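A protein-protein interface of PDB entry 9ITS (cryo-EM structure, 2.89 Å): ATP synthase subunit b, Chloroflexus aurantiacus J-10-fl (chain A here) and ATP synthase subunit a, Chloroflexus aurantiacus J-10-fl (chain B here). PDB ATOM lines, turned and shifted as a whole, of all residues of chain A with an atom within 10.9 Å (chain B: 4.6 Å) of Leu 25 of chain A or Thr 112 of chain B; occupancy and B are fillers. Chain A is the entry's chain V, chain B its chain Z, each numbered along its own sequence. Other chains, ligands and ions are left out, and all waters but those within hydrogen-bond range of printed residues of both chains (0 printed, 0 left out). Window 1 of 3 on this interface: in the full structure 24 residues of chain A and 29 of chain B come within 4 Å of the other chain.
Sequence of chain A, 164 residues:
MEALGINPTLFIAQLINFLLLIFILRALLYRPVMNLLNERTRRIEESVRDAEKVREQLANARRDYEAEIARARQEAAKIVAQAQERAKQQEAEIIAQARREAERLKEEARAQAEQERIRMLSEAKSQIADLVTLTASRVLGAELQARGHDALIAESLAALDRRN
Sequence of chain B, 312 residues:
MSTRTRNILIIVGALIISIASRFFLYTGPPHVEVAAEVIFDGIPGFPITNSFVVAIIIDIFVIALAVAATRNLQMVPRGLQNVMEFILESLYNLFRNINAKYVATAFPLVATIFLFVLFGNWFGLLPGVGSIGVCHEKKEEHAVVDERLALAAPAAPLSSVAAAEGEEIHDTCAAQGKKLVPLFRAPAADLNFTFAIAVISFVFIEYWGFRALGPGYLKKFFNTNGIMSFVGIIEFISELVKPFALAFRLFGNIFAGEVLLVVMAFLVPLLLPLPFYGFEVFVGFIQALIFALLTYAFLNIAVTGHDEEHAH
The side-chain hydroxyl (OG1) of Thr 112 of chain B sits at hydrogen-bond distance from the backbone carbonyl oxygen (O) of Pro 108 of chain B.
The backbone carbonyl oxygen of Leu 109 of chain B is in hydrogen-bond range of the side-chain hydroxyl of Thr 112 of chain B, at 2.6 Å.
N of Arg 31 of chain A sits close to O of Arg 26 of chain A, 3.5 Å away.
Printed residues of chain A that touch a printed residue of chain B: Phe 18, Ile 22, Ile 24, Leu 25, Arg 26, Leu 28, Leu 29 and Tyr 30.
Hydrophobic or aromatic side chains of chain A that line the printed part of chain B: Phe 18, Ile 22, Ile 24, Leu 25, Leu 28, Leu 29 and Tyr 30.
Of the 12 printed residues of chain B, 9 touch a printed residue of chain A.
Of the printed residues of chain B, Phe 18 of chain A touches Ile 113 and Phe 116.
Leu 19 of chain A touches none of the printed residues of chain B.
Of the printed residues of chain B, Ile 22 of chain A touches Thr 112.
Leu 25 of chain A touches just these residues of chain B: Val 62, Ile 63 and Thr 112.
Printed residues of chain A within 4 Å of Val 62 of chain B: Leu 25.
Ile 63 of chain B touches just these residues of chain A: Ile 24 (3.9 Å), Leu 25 (3.7 Å) and Leu 28 (3.8 Å).
Leu 109 of chain B touches none of the printed residues of chain A.
Thr 112 of chain B touches three residues of chain A.
Ile 113 of chain B touches just one residue of chain A: Phe 18 (3.7 Å).
Phe 114 of chain B touches none of the printed residues of chain A.
Leu 115 of chain B touches one residue of chain A.
The nearest printed residue of chain B that does not touch Arg 26 of chain A is Thr 112 of chain B (5.1 Å).
Among the printed residues, pairs that only touch across the chains: Ile 22 of chain A with Thr 112 of chain B, Tyr 30 of chain A with Leu 115 of chain B, Tyr 30 of chain A with Ala 111 of chain B, Tyr 30 of chain A with Pro 108 of chain B, Phe 18 of chain A with Phe 116 of chain B, Arg 26 of chain A with Pro 108 of chain B, Leu 25 of chain A with Val 62 of chain B, Phe 18 of chain A with Ile 113 of chain B, Leu 25 of chain A with Ile 63 of chain B, Leu 28 of chain A with Ala 66 of chain B, Leu 29 of chain A with Ala 66 of chain B, Leu 28 of chain A with Ile 63 of chain B, Ile 24 of chain A with Ile 63 of chain B and Leu 25 of chain A with Thr 112 of chain B.
OH of Tyr 30 of chain A lies within hydrogen-bond range of N of Thr 112 of chain B.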
ATOM      1  N   LEU A  15     -10.522   2.317  22.834  1.00  0.00           N
ATOM      2  CA  LEU A  15      -9.545   1.832  21.863  1.00  0.00           C
ATOM      3  C   LEU A  15     -10.223   1.087  20.718  1.00  0.00           C
ATOM      4  O   LEU A  15      -9.905   1.313  19.546  1.00  0.00           O
ATOM      5  CB  LEU A  15      -8.522   0.940  22.569  1.00  0.00           C
ATOM      6  CG  LEU A  15      -7.281   0.433  21.832  1.00  0.00           C
ATOM      7  CD1 LEU A  15      -6.120   0.351  22.799  1.00  0.00           C
ATOM      8  CD2 LEU A  15      -7.533  -0.936  21.227  1.00  0.00           C
ATOM      9  N   ILE A  16     -11.171   0.204  21.039  1.00  0.00           N
ATOM     10  CA  ILE A  16     -11.883  -0.546  20.010  1.00  0.00           C
ATOM     11  C   ILE A  16     -12.720   0.395  19.153  1.00  0.00           C
ATOM     12  O   ILE A  16     -12.837   0.213  17.935  1.00  0.00           O
ATOM     13  CB  ILE A  16     -12.736  -1.652  20.660  1.00  0.00           C
ATOM     14  CG1 ILE A  16     -11.833  -2.755  21.215  1.00  0.00           C
ATOM     15  CG2 ILE A  16     -13.734  -2.239  19.672  1.00  0.00           C
ATOM     16  CD1 ILE A  16     -11.023  -3.469  20.155  1.00  0.00           C
ATOM     17  N   ASN A  17     -13.303   1.425  19.775  1.00  0.00           N
ATOM     18  CA  ASN A  17     -14.017   2.446  19.018  1.00  0.00           C
ATOM     19  C   ASN A  17     -13.094   3.124  18.009  1.00  0.00           C
ATOM     20  O   ASN A  17     -13.459   3.307  16.840  1.00  0.00           O
ATOM     21  CB  ASN A  17     -14.609   3.472  19.987  1.00  0.00           C
ATOM     22  CG  ASN A  17     -15.424   4.539  19.290  1.00  0.00           C
ATOM     23  OD1 ASN A  17     -15.912   4.336  18.183  1.00  0.00           O
ATOM     24  ND2 ASN A  17     -15.569   5.690  19.935  1.00  0.00           N
ATOM     25  N   PHE A  18     -11.881   3.482  18.443  1.00  0.00           N
ATOM     26  CA  PHE A  18     -10.931   4.121  17.536  1.00  0.00           C
ATOM     27  C   PHE A  18     -10.514   3.187  16.405  1.00  0.00           C
ATOM     28  O   PHE A  18     -10.396   3.620  15.254  1.00  0.00           O
ATOM     29  CB  PHE A  18      -9.706   4.608  18.309  1.00  0.00           C
ATOM     30  CG  PHE A  18      -8.892   5.628  17.565  1.00  0.00           C
ATOM     31  CD1 PHE A  18      -9.479   6.792  17.095  1.00  0.00           C
ATOM     32  CD2 PHE A  18      -7.543   5.421  17.328  1.00  0.00           C
ATOM     33  CE1 PHE A  18      -8.736   7.732  16.406  1.00  0.00           C
ATOM     34  CE2 PHE A  18      -6.794   6.357  16.640  1.00  0.00           C
ATOM     35  CZ  PHE A  18      -7.392   7.514  16.179  1.00  0.00           C
ATOM     36  N   LEU A  19     -10.278   1.906  16.712  1.00  0.00           N
ATOM     37  CA  LEU A  19      -9.942   0.947  15.658  1.00  0.00           C
ATOM     38  C   LEU A  19     -11.076   0.799  14.651  1.00  0.00           C
ATOM     39  O   LEU A  19     -10.835   0.733  13.439  1.00  0.00           O
ATOM     40  CB  LEU A  19      -9.582  -0.419  16.249  1.00  0.00           C
ATOM     41  CG  LEU A  19      -8.148  -0.723  16.704  1.00  0.00           C
ATOM     42  CD1 LEU A  19      -7.211  -0.678  15.505  1.00  0.00           C
ATOM     43  CD2 LEU A  19      -7.653   0.209  17.781  1.00  0.00           C
ATOM     44  N   LEU A  20     -12.320   0.745  15.131  1.00  0.00           N
ATOM     45  CA  LEU A  20     -13.453   0.653  14.216  1.00  0.00           C
ATOM     46  C   LEU A  20     -13.537   1.882  13.320  1.00  0.00           C
ATOM     47  O   LEU A  20     -13.790   1.760  12.116  1.00  0.00           O
ATOM     48  CB  LEU A  20     -14.754   0.461  14.996  1.00  0.00           C
ATOM     49  CG  LEU A  20     -15.271  -0.978  15.091  1.00  0.00           C
ATOM     50  CD1 LEU A  20     -14.345  -1.850  15.924  1.00  0.00           C
ATOM     51  CD2 LEU A  20     -16.686  -1.001  15.650  1.00  0.00           C
ATOM     52  N   LEU A  21     -13.316   3.071  13.885  1.00  0.00           N
ATOM     53  CA  LEU A  21     -13.334   4.282  13.066  1.00  0.00           C
ATOM     54  C   LEU A  21     -12.213   4.295  12.033  1.00  0.00           C
ATOM     55  O   LEU A  21     -12.444   4.649  10.873  1.00  0.00           O
ATOM     56  CB  LEU A  21     -13.284   5.538  13.937  1.00  0.00           C
ATOM     57  CG  LEU A  21     -14.632   6.077  14.421  1.00  0.00           C
ATOM     58  CD1 LEU A  21     -15.420   6.541  13.209  1.00  0.00           C
ATOM     59  CD2 LEU A  21     -15.453   5.069  15.183  1.00  0.00           C
ATOM     60  N   ILE A  22     -10.993   3.917  12.423  1.00  0.00           N
ATOM     61  CA  ILE A  22      -9.913   3.947  11.437  1.00  0.00           C
ATOM     62  C   ILE A  22     -10.161   2.914  10.342  1.00  0.00           C
ATOM     63  O   ILE A  22      -9.866   3.167   9.166  1.00  0.00           O
ATOM     64  CB  ILE A  22      -8.524   3.778  12.093  1.00  0.00           C
ATOM     65  CG1 ILE A  22      -8.277   2.346  12.571  1.00  0.00           C
ATOM     66  CG2 ILE A  22      -8.331   4.771  13.227  1.00  0.00           C
ATOM     67  CD1 ILE A  22      -6.838   2.066  12.938  1.00  0.00           C
ATOM     68  N   PHE A  23     -10.747   1.764  10.688  1.00  0.00           N
ATOM     69  CA  PHE A  23     -11.002   0.743   9.678  1.00  0.00           C
ATOM     70  C   PHE A  23     -12.127   1.153   8.733  1.00  0.00           C
ATOM     71  O   PHE A  23     -12.040   0.913   7.523  1.00  0.00           O
ATOM     72  CB  PHE A  23     -11.315  -0.591  10.352  1.00  0.00           C
ATOM     73  CG  PHE A  23     -10.099  -1.289  10.891  1.00  0.00           C
ATOM     74  CD1 PHE A  23      -8.854  -1.072  10.324  1.00  0.00           C
ATOM     75  CD2 PHE A  23     -10.198  -2.156  11.967  1.00  0.00           C
ATOM     76  CE1 PHE A  23      -7.731  -1.707  10.816  1.00  0.00           C
ATOM     77  CE2 PHE A  23      -9.078  -2.796  12.464  1.00  0.00           C
ATOM     78  CZ  PHE A  23      -7.842  -2.571  11.888  1.00  0.00           C
ATOM     79  N   ILE A  24     -13.196   1.762   9.256  1.00  0.00           N
ATOM     80  CA  ILE A  24     -14.281   2.165   8.367  1.00  0.00           C
ATOM     81  C   ILE A  24     -13.887   3.379   7.532  1.00  0.00           C
ATOM     82  O   ILE A  24     -14.318   3.507   6.381  1.00  0.00           O
ATOM     83  CB  ILE A  24     -15.591   2.406   9.146  1.00  0.00           C
ATOM     84  CG1 ILE A  24     -15.470   3.593  10.104  1.00  0.00           C
ATOM     85  CG2 ILE A  24     -16.023   1.138   9.875  1.00  0.00           C
ATOM     86  CD1 ILE A  24     -16.705   3.825  10.945  1.00  0.00           C
ATOM     87  N   LEU A  25     -13.064   4.283   8.074  1.00  0.00           N
ATOM     88  CA  LEU A  25     -12.643   5.447   7.303  1.00  0.00           C
ATOM     89  C   LEU A  25     -11.600   5.094   6.249  1.00  0.00           C
ATOM     90  O   LEU A  25     -11.596   5.694   5.170  1.00  0.00           O
ATOM     91  CB  LEU A  25     -12.106   6.540   8.232  1.00  0.00           C
ATOM     92  CG  LEU A  25     -13.081   7.578   8.810  1.00  0.00           C
ATOM     93  CD1 LEU A  25     -13.676   8.417   7.697  1.00  0.00           C
ATOM     94  CD2 LEU A  25     -14.192   6.968   9.646  1.00  0.00           C
ATOM     95  N   ARG A  26     -10.712   4.136   6.533  1.00  0.00           N
ATOM     96  CA  ARG A  26      -9.731   3.730   5.535  1.00  0.00           C
ATOM     97  C   ARG A  26     -10.361   2.983   4.366  1.00  0.00           C
ATOM     98  O   ARG A  26      -9.745   2.902   3.297  1.00  0.00           O
ATOM     99  CB  ARG A  26      -8.641   2.865   6.173  1.00  0.00           C
ATOM    100  CG  ARG A  26      -9.041   1.423   6.430  1.00  0.00           C
ATOM    101  CD  ARG A  26      -7.836   0.502   6.368  1.00  0.00           C
ATOM    102  NE  ARG A  26      -7.421   0.239   4.995  1.00  0.00           N
ATOM    103  CZ  ARG A  26      -6.164   0.074   4.611  1.00  0.00           C
ATOM    104  NH1 ARG A  26      -5.162   0.138   5.472  1.00  0.00           N
ATOM    105  NH2 ARG A  26      -5.904  -0.161   3.328  1.00  0.00           N
ATOM    106  N   ALA A  27     -11.564   2.440   4.542  1.00  0.00           N
ATOM    107  CA  ALA A  27     -12.260   1.734   3.477  1.00  0.00           C
ATOM    108  C   ALA A  27     -13.402   2.539   2.869  1.00  0.00           C
ATOM    109  O   ALA A  27     -14.066   2.043   1.953  1.00  0.00           O
ATOM    110  CB  ALA A  27     -12.799   0.396   3.995  1.00  0.00           C
ATOM    111  N   LEU A  28     -13.648   3.759   3.349  1.00  0.00           N
ATOM    112  CA  LEU A  28     -14.735   4.590   2.839  1.00  0.00           C
ATOM    113  C   LEU A  28     -14.244   5.612   1.821  1.00  0.00           C
ATOM    114  O   LEU A  28     -14.731   5.647   0.688  1.00  0.00           O
ATOM    115  CB  LEU A  28     -15.450   5.300   3.996  1.00  0.00           C
ATOM    116  CG  LEU A  28     -16.651   6.163   3.605  1.00  0.00           C
ATOM    117  CD1 LEU A  28     -17.740   5.315   2.966  1.00  0.00           C
ATOM    118  CD2 LEU A  28     -17.190   6.916   4.811  1.00  0.00           C
ATOM    119  N   LEU A  29     -13.285   6.455   2.207  1.00  0.00           N
ATOM    120  CA  LEU A  29     -12.783   7.495   1.324  1.00  0.00           C
ATOM    121  C   LEU A  29     -11.279   7.461   1.115  1.00  0.00           C
ATOM    122  O   LEU A  29     -10.813   7.972   0.092  1.00  0.00           O
ATOM    123  CB  LEU A  29     -13.162   8.892   1.846  1.00  0.00           C
ATOM    124  CG  LEU A  29     -12.348   9.506   2.989  1.00  0.00           C
ATOM    125  CD1 LEU A  29     -12.628  10.999   3.098  1.00  0.00           C
ATOM    126  CD2 LEU A  29     -12.620   8.820   4.310  1.00  0.00           C
ATOM    127  N   TYR A  30     -10.509   6.877   2.038  1.00  0.00           N
ATOM    128  CA  TYR A  30      -9.056   6.877   1.889  1.00  0.00           C
ATOM    129  C   TYR A  30      -8.624   6.088   0.661  1.00  0.00           C
ATOM    130  O   TYR A  30      -7.802   6.561  -0.131  1.00  0.00           O
ATOM    131  CB  TYR A  30      -8.394   6.311   3.144  1.00  0.00           C
ATOM    132  CG  TYR A  30      -8.395   7.252   4.327  1.00  0.00           C
ATOM    133  CD1 TYR A  30      -8.850   8.558   4.206  1.00  0.00           C
ATOM    134  CD2 TYR A  30      -7.924   6.835   5.564  1.00  0.00           C
ATOM    135  CE1 TYR A  30      -8.849   9.417   5.288  1.00  0.00           C
ATOM    136  CE2 TYR A  30      -7.917   7.684   6.647  1.00  0.00           C
ATOM    137  CZ  TYR A  30      -8.381   8.974   6.506  1.00  0.00           C
ATOM    138  OH  TYR A  30      -8.373   9.822   7.590  1.00  0.00           O
ATOM    139  N   ARG A  31      -9.164   4.876   0.490  1.00  0.00           N
ATOM    140  CA  ARG A  31      -8.855   4.107  -0.714  1.00  0.00           C
ATOM    141  C   ARG A  31      -9.383   4.771  -1.984  1.00  0.00           C
ATOM    142  O   ARG A  31      -8.633   4.827  -2.975  1.00  0.00           O
ATOM    143  CB  ARG A  31      -9.355   2.666  -0.558  1.00  0.00           C
ATOM    144  CG  ARG A  31      -8.480   1.802   0.332  1.00  0.00           C
ATOM    145  CD  ARG A  31      -7.165   1.462  -0.351  1.00  0.00           C
ATOM    146  NE  ARG A  31      -6.495   0.331   0.281  1.00  0.00           N
ATOM    147  CZ  ARG A  31      -6.830  -0.938   0.096  1.00  0.00           C
ATOM    148  NH1 ARG A  31      -7.823  -1.283  -0.708  1.00  0.00           N
ATOM    149  NH2 ARG A  31      -6.147  -1.888   0.730  1.00  0.00           N
ATOM    150  N   PRO A  32     -10.636   5.257  -2.052  1.00  0.00           N
ATOM    151  CA  PRO A  32     -11.046   5.991  -3.266  1.00  0.00           C
ATOM    152  C   PRO A  32     -10.207   7.224  -3.565  1.00  0.00           C
ATOM    153  O   PRO A  32      -9.899   7.476  -4.734  1.00  0.00           O
ATOM    154  CB  PRO A  32     -12.505   6.360  -2.971  1.00  0.00           C
ATOM    155  CG  PRO A  32     -12.974   5.306  -2.061  1.00  0.00           C
ATOM    156  CD  PRO A  32     -11.801   4.977  -1.189  1.00  0.00           C
ATOM    157  N   VAL A  33      -9.812   7.992  -2.547  1.00  0.00           N
ATOM    158  CA  VAL A  33      -9.013   9.190  -2.799  1.00  0.00           C
ATOM    159  C   VAL A  33      -7.605   8.811  -3.249  1.00  0.00           C
ATOM    160  O   VAL A  33      -7.038   9.439  -4.152  1.00  0.00           O
ATOM    161  CB  VAL A  33      -8.998  10.096  -1.554  1.00  0.00           C
ATOM    162  CG1 VAL A  33      -7.905  11.148  -1.658  1.00  0.00           C
ATOM    163  CG2 VAL A  33     -10.349  10.767  -1.388  1.00  0.00           C
ATOM    164  N   MET A  34      -7.026   7.774  -2.639  1.00  0.00           N
ATOM    165  CA  MET A  34      -5.714   7.303  -3.067  1.00  0.00           C
ATOM    166  C   MET A  34      -5.755   6.796  -4.504  1.00  0.00           C
ATOM    167  O   MET A  34      -4.846   7.073  -5.296  1.00  0.00           O
ATOM    168  CB  MET A  34      -5.219   6.208  -2.123  1.00  0.00           C
ATOM    169  CG  MET A  34      -3.803   5.735  -2.403  1.00  0.00           C
ATOM    170  SD  MET A  34      -2.563   6.985  -2.013  1.00  0.00           S
ATOM    171  CE  MET A  34      -1.219   6.470  -3.079  1.00  0.00           C
ATOM    172  N   VAL B  62     -17.548  13.078  10.900  1.00  0.00           N
ATOM    173  CA  VAL B  62     -16.503  12.672   9.967  1.00  0.00           C
ATOM    174  C   VAL B  62     -17.068  11.741   8.903  1.00  0.00           C
ATOM    175  O   VAL B  62     -16.761  11.883   7.713  1.00  0.00           O
ATOM    176  CB  VAL B  62     -15.331  12.028  10.732  1.00  0.00           C
ATOM    177  CG1 VAL B  62     -14.397  11.306   9.781  1.00  0.00           C
ATOM    178  CG2 VAL B  62     -14.568  13.084  11.512  1.00  0.00           C
ATOM    179  N   ILE B  63     -17.911  10.787   9.306  1.00  0.00           N
ATOM    180  CA  ILE B  63     -18.537   9.887   8.343  1.00  0.00           C
ATOM    181  C   ILE B  63     -19.429  10.670   7.385  1.00  0.00           C
ATOM    182  O   ILE B  63     -19.442  10.412   6.174  1.00  0.00           O
ATOM    183  CB  ILE B  63     -19.316   8.781   9.081  1.00  0.00           C
ATOM    184  CG1 ILE B  63     -18.351   7.733   9.641  1.00  0.00           C
ATOM    185  CG2 ILE B  63     -20.346   8.127   8.168  1.00  0.00           C
ATOM    186  CD1 ILE B  63     -17.780   6.802   8.592  1.00  0.00           C
ATOM    187  N   ALA B  66     -17.237  12.607   4.952  1.00  0.00           N
ATOM    188  CA  ALA B  66     -16.589  11.675   4.037  1.00  0.00           C
ATOM    189  C   ALA B  66     -17.559  11.167   2.978  1.00  0.00           C
ATOM    190  O   ALA B  66     -17.207  11.086   1.796  1.00  0.00           O
ATOM    191  CB  ALA B  66     -15.988  10.507   4.818  1.00  0.00           C
ATOM    192  N   PRO B 108      -3.355   5.707   6.301  1.00  0.00           N
ATOM    193  CA  PRO B 108      -4.715   5.772   6.869  1.00  0.00           C
ATOM    194  C   PRO B 108      -4.736   5.943   8.377  1.00  0.00           C
ATOM    195  O   PRO B 108      -5.543   6.731   8.891  1.00  0.00           O
ATOM    196  CB  PRO B 108      -5.342   4.439   6.436  1.00  0.00           C
ATOM    197  CG  PRO B 108      -4.191   3.541   6.191  1.00  0.00           C
ATOM    198  CD  PRO B 108      -3.138   4.423   5.607  1.00  0.00           C
ATOM    199  N   LEU B 109      -3.855   5.247   9.100  1.00  0.00           N
ATOM    200  CA  LEU B 109      -3.834   5.355  10.555  1.00  0.00           C
ATOM    201  C   LEU B 109      -3.463   6.763  11.001  1.00  0.00           C
ATOM    202  O   LEU B 109      -4.127   7.338  11.874  1.00  0.00           O
ATOM    203  CB  LEU B 109      -2.863   4.328  11.140  1.00  0.00           C
ATOM    204  CG  LEU B 109      -2.847   4.132  12.658  1.00  0.00           C
ATOM    205  CD1 LEU B 109      -2.701   2.659  12.993  1.00  0.00           C
ATOM    206  CD2 LEU B 109      -1.723   4.931  13.303  1.00  0.00           C
ATOM    207  N   VAL B 110      -2.416   7.338  10.408  1.00  0.00           N
ATOM    208  CA  VAL B 110      -1.981   8.673  10.803  1.00  0.00           C
ATOM    209  C   VAL B 110      -3.007   9.721  10.381  1.00  0.00           C
ATOM    210  O   VAL B 110      -3.268  10.681  11.114  1.00  0.00           O
ATOM    211  CB  VAL B 110      -0.583   8.970  10.229  1.00  0.00           C
ATOM    212  CG1 VAL B 110      -0.113  10.340  10.665  1.00  0.00           C
ATOM    213  CG2 VAL B 110       0.406   7.914  10.691  1.00  0.00           C
ATOM    214  N   ALA B 111      -3.620   9.544   9.208  1.00  0.00           N
ATOM    215  CA  ALA B 111      -4.647  10.481   8.764  1.00  0.00           C
ATOM    216  C   ALA B 111      -5.853  10.467   9.696  1.00  0.00           C
ATOM    217  O   ALA B 111      -6.392  11.526  10.043  1.00  0.00           O
ATOM    218  CB  ALA B 111      -5.070  10.155   7.332  1.00  0.00           C
ATOM    219  N   THR B 112      -6.291   9.276  10.115  1.00  0.00           N
ATOM    220  CA  THR B 112      -7.397   9.190  11.064  1.00  0.00           C
ATOM    221  C   THR B 112      -7.022   9.780  12.417  1.00  0.00           C
ATOM    222  O   THR B 112      -7.804  10.532  13.009  1.00  0.00           O
ATOM    223  CB  THR B 112      -7.837   7.737  11.230  1.00  0.00           C
ATOM    224  OG1 THR B 112      -6.683   6.900  11.366  1.00  0.00           O
ATOM    225  CG2 THR B 112      -8.662   7.283  10.042  1.00  0.00           C
ATOM    226  N   ILE B 113      -5.831   9.448  12.925  1.00  0.00           N
ATOM    227  CA  ILE B 113      -5.407   9.947  14.229  1.00  0.00           C
ATOM    228  C   ILE B 113      -5.137  11.442  14.203  1.00  0.00           C
ATOM    229  O   ILE B 113      -5.068  12.072  15.261  1.00  0.00           O
ATOM    230  CB  ILE B 113      -4.169   9.163  14.715  1.00  0.00           C
ATOM    231  CG1 ILE B 113      -4.082   9.168  16.240  1.00  0.00           C
ATOM    232  CG2 ILE B 113      -2.892   9.759  14.158  1.00  0.00           C
ATOM    233  CD1 ILE B 113      -3.134   8.121  16.782  1.00  0.00           C
ATOM    234  N   PHE B 114      -4.979  12.022  13.012  1.00  0.00           N
ATOM    235  CA  PHE B 114      -4.885  13.469  12.873  1.00  0.00           C
ATOM    236  C   PHE B 114      -6.268  14.108  12.828  1.00  0.00           C
ATOM    237  O   PHE B 114      -6.550  15.045  13.583  1.00  0.00           O
ATOM    238  CB  PHE B 114      -4.085  13.809  11.613  1.00  0.00           C
ATOM    239  CG  PHE B 114      -4.281  15.215  11.121  1.00  0.00           C
ATOM    240  CD1 PHE B 114      -3.652  16.276  11.747  1.00  0.00           C
ATOM    241  CD2 PHE B 114      -5.082  15.473  10.020  1.00  0.00           C
ATOM    242  CE1 PHE B 114      -3.827  17.569  11.292  1.00  0.00           C
ATOM    243  CE2 PHE B 114      -5.261  16.762   9.561  1.00  0.00           C
ATOM    244  CZ  PHE B 114      -4.630  17.811  10.197  1.00  0.00           C
ATOM    245  N   LEU B 115      -7.143  13.605  11.951  1.00  0.00           N
ATOM    246  CA  LEU B 115      -8.456  14.218  11.759  1.00  0.00           C
ATOM    247  C   LEU B 115      -9.324  14.106  13.006  1.00  0.00           C
ATOM    248  O   LEU B 115     -10.034  15.058  13.363  1.00  0.00           O
ATOM    249  CB  LEU B 115      -9.159  13.579  10.562  1.00  0.00           C
ATOM    250  CG  LEU B 115      -8.589  13.926   9.186  1.00  0.00           C
ATOM    251  CD1 LEU B 115      -9.148  12.993   8.125  1.00  0.00           C
ATOM    252  CD2 LEU B 115      -8.884  15.375   8.839  1.00  0.00           C
ATOM    253  N   PHE B 116      -9.294  12.948  13.675  1.00  0.00           N
ATOM    254  CA  PHE B 116     -10.126  12.752  14.857  1.00  0.00           C
ATOM    255  C   PHE B 116      -9.743  13.719  15.969  1.00  0.00           C
ATOM    256  O   PHE B 116     -10.610  14.371  16.561  1.00  0.00           O
ATOM    257  CB  PHE B 116     -10.016  11.305  15.340  1.00  0.00           C
ATOM    258  CG  PHE B 116     -11.055  10.928  16.354  1.00  0.00           C
ATOM    259  CD1 PHE B 116     -12.400  11.088  16.076  1.00  0.00           C
ATOM    260  CD2 PHE B 116     -10.685  10.413  17.584  1.00  0.00           C
ATOM    261  CE1 PHE B 116     -13.358  10.744  17.010  1.00  0.00           C
ATOM    262  CE2 PHE B 116     -11.641  10.066  18.520  1.00  0.00           C
ATOM    263  CZ  PHE B 116     -12.978  10.231  18.231  1.00  0.00           C
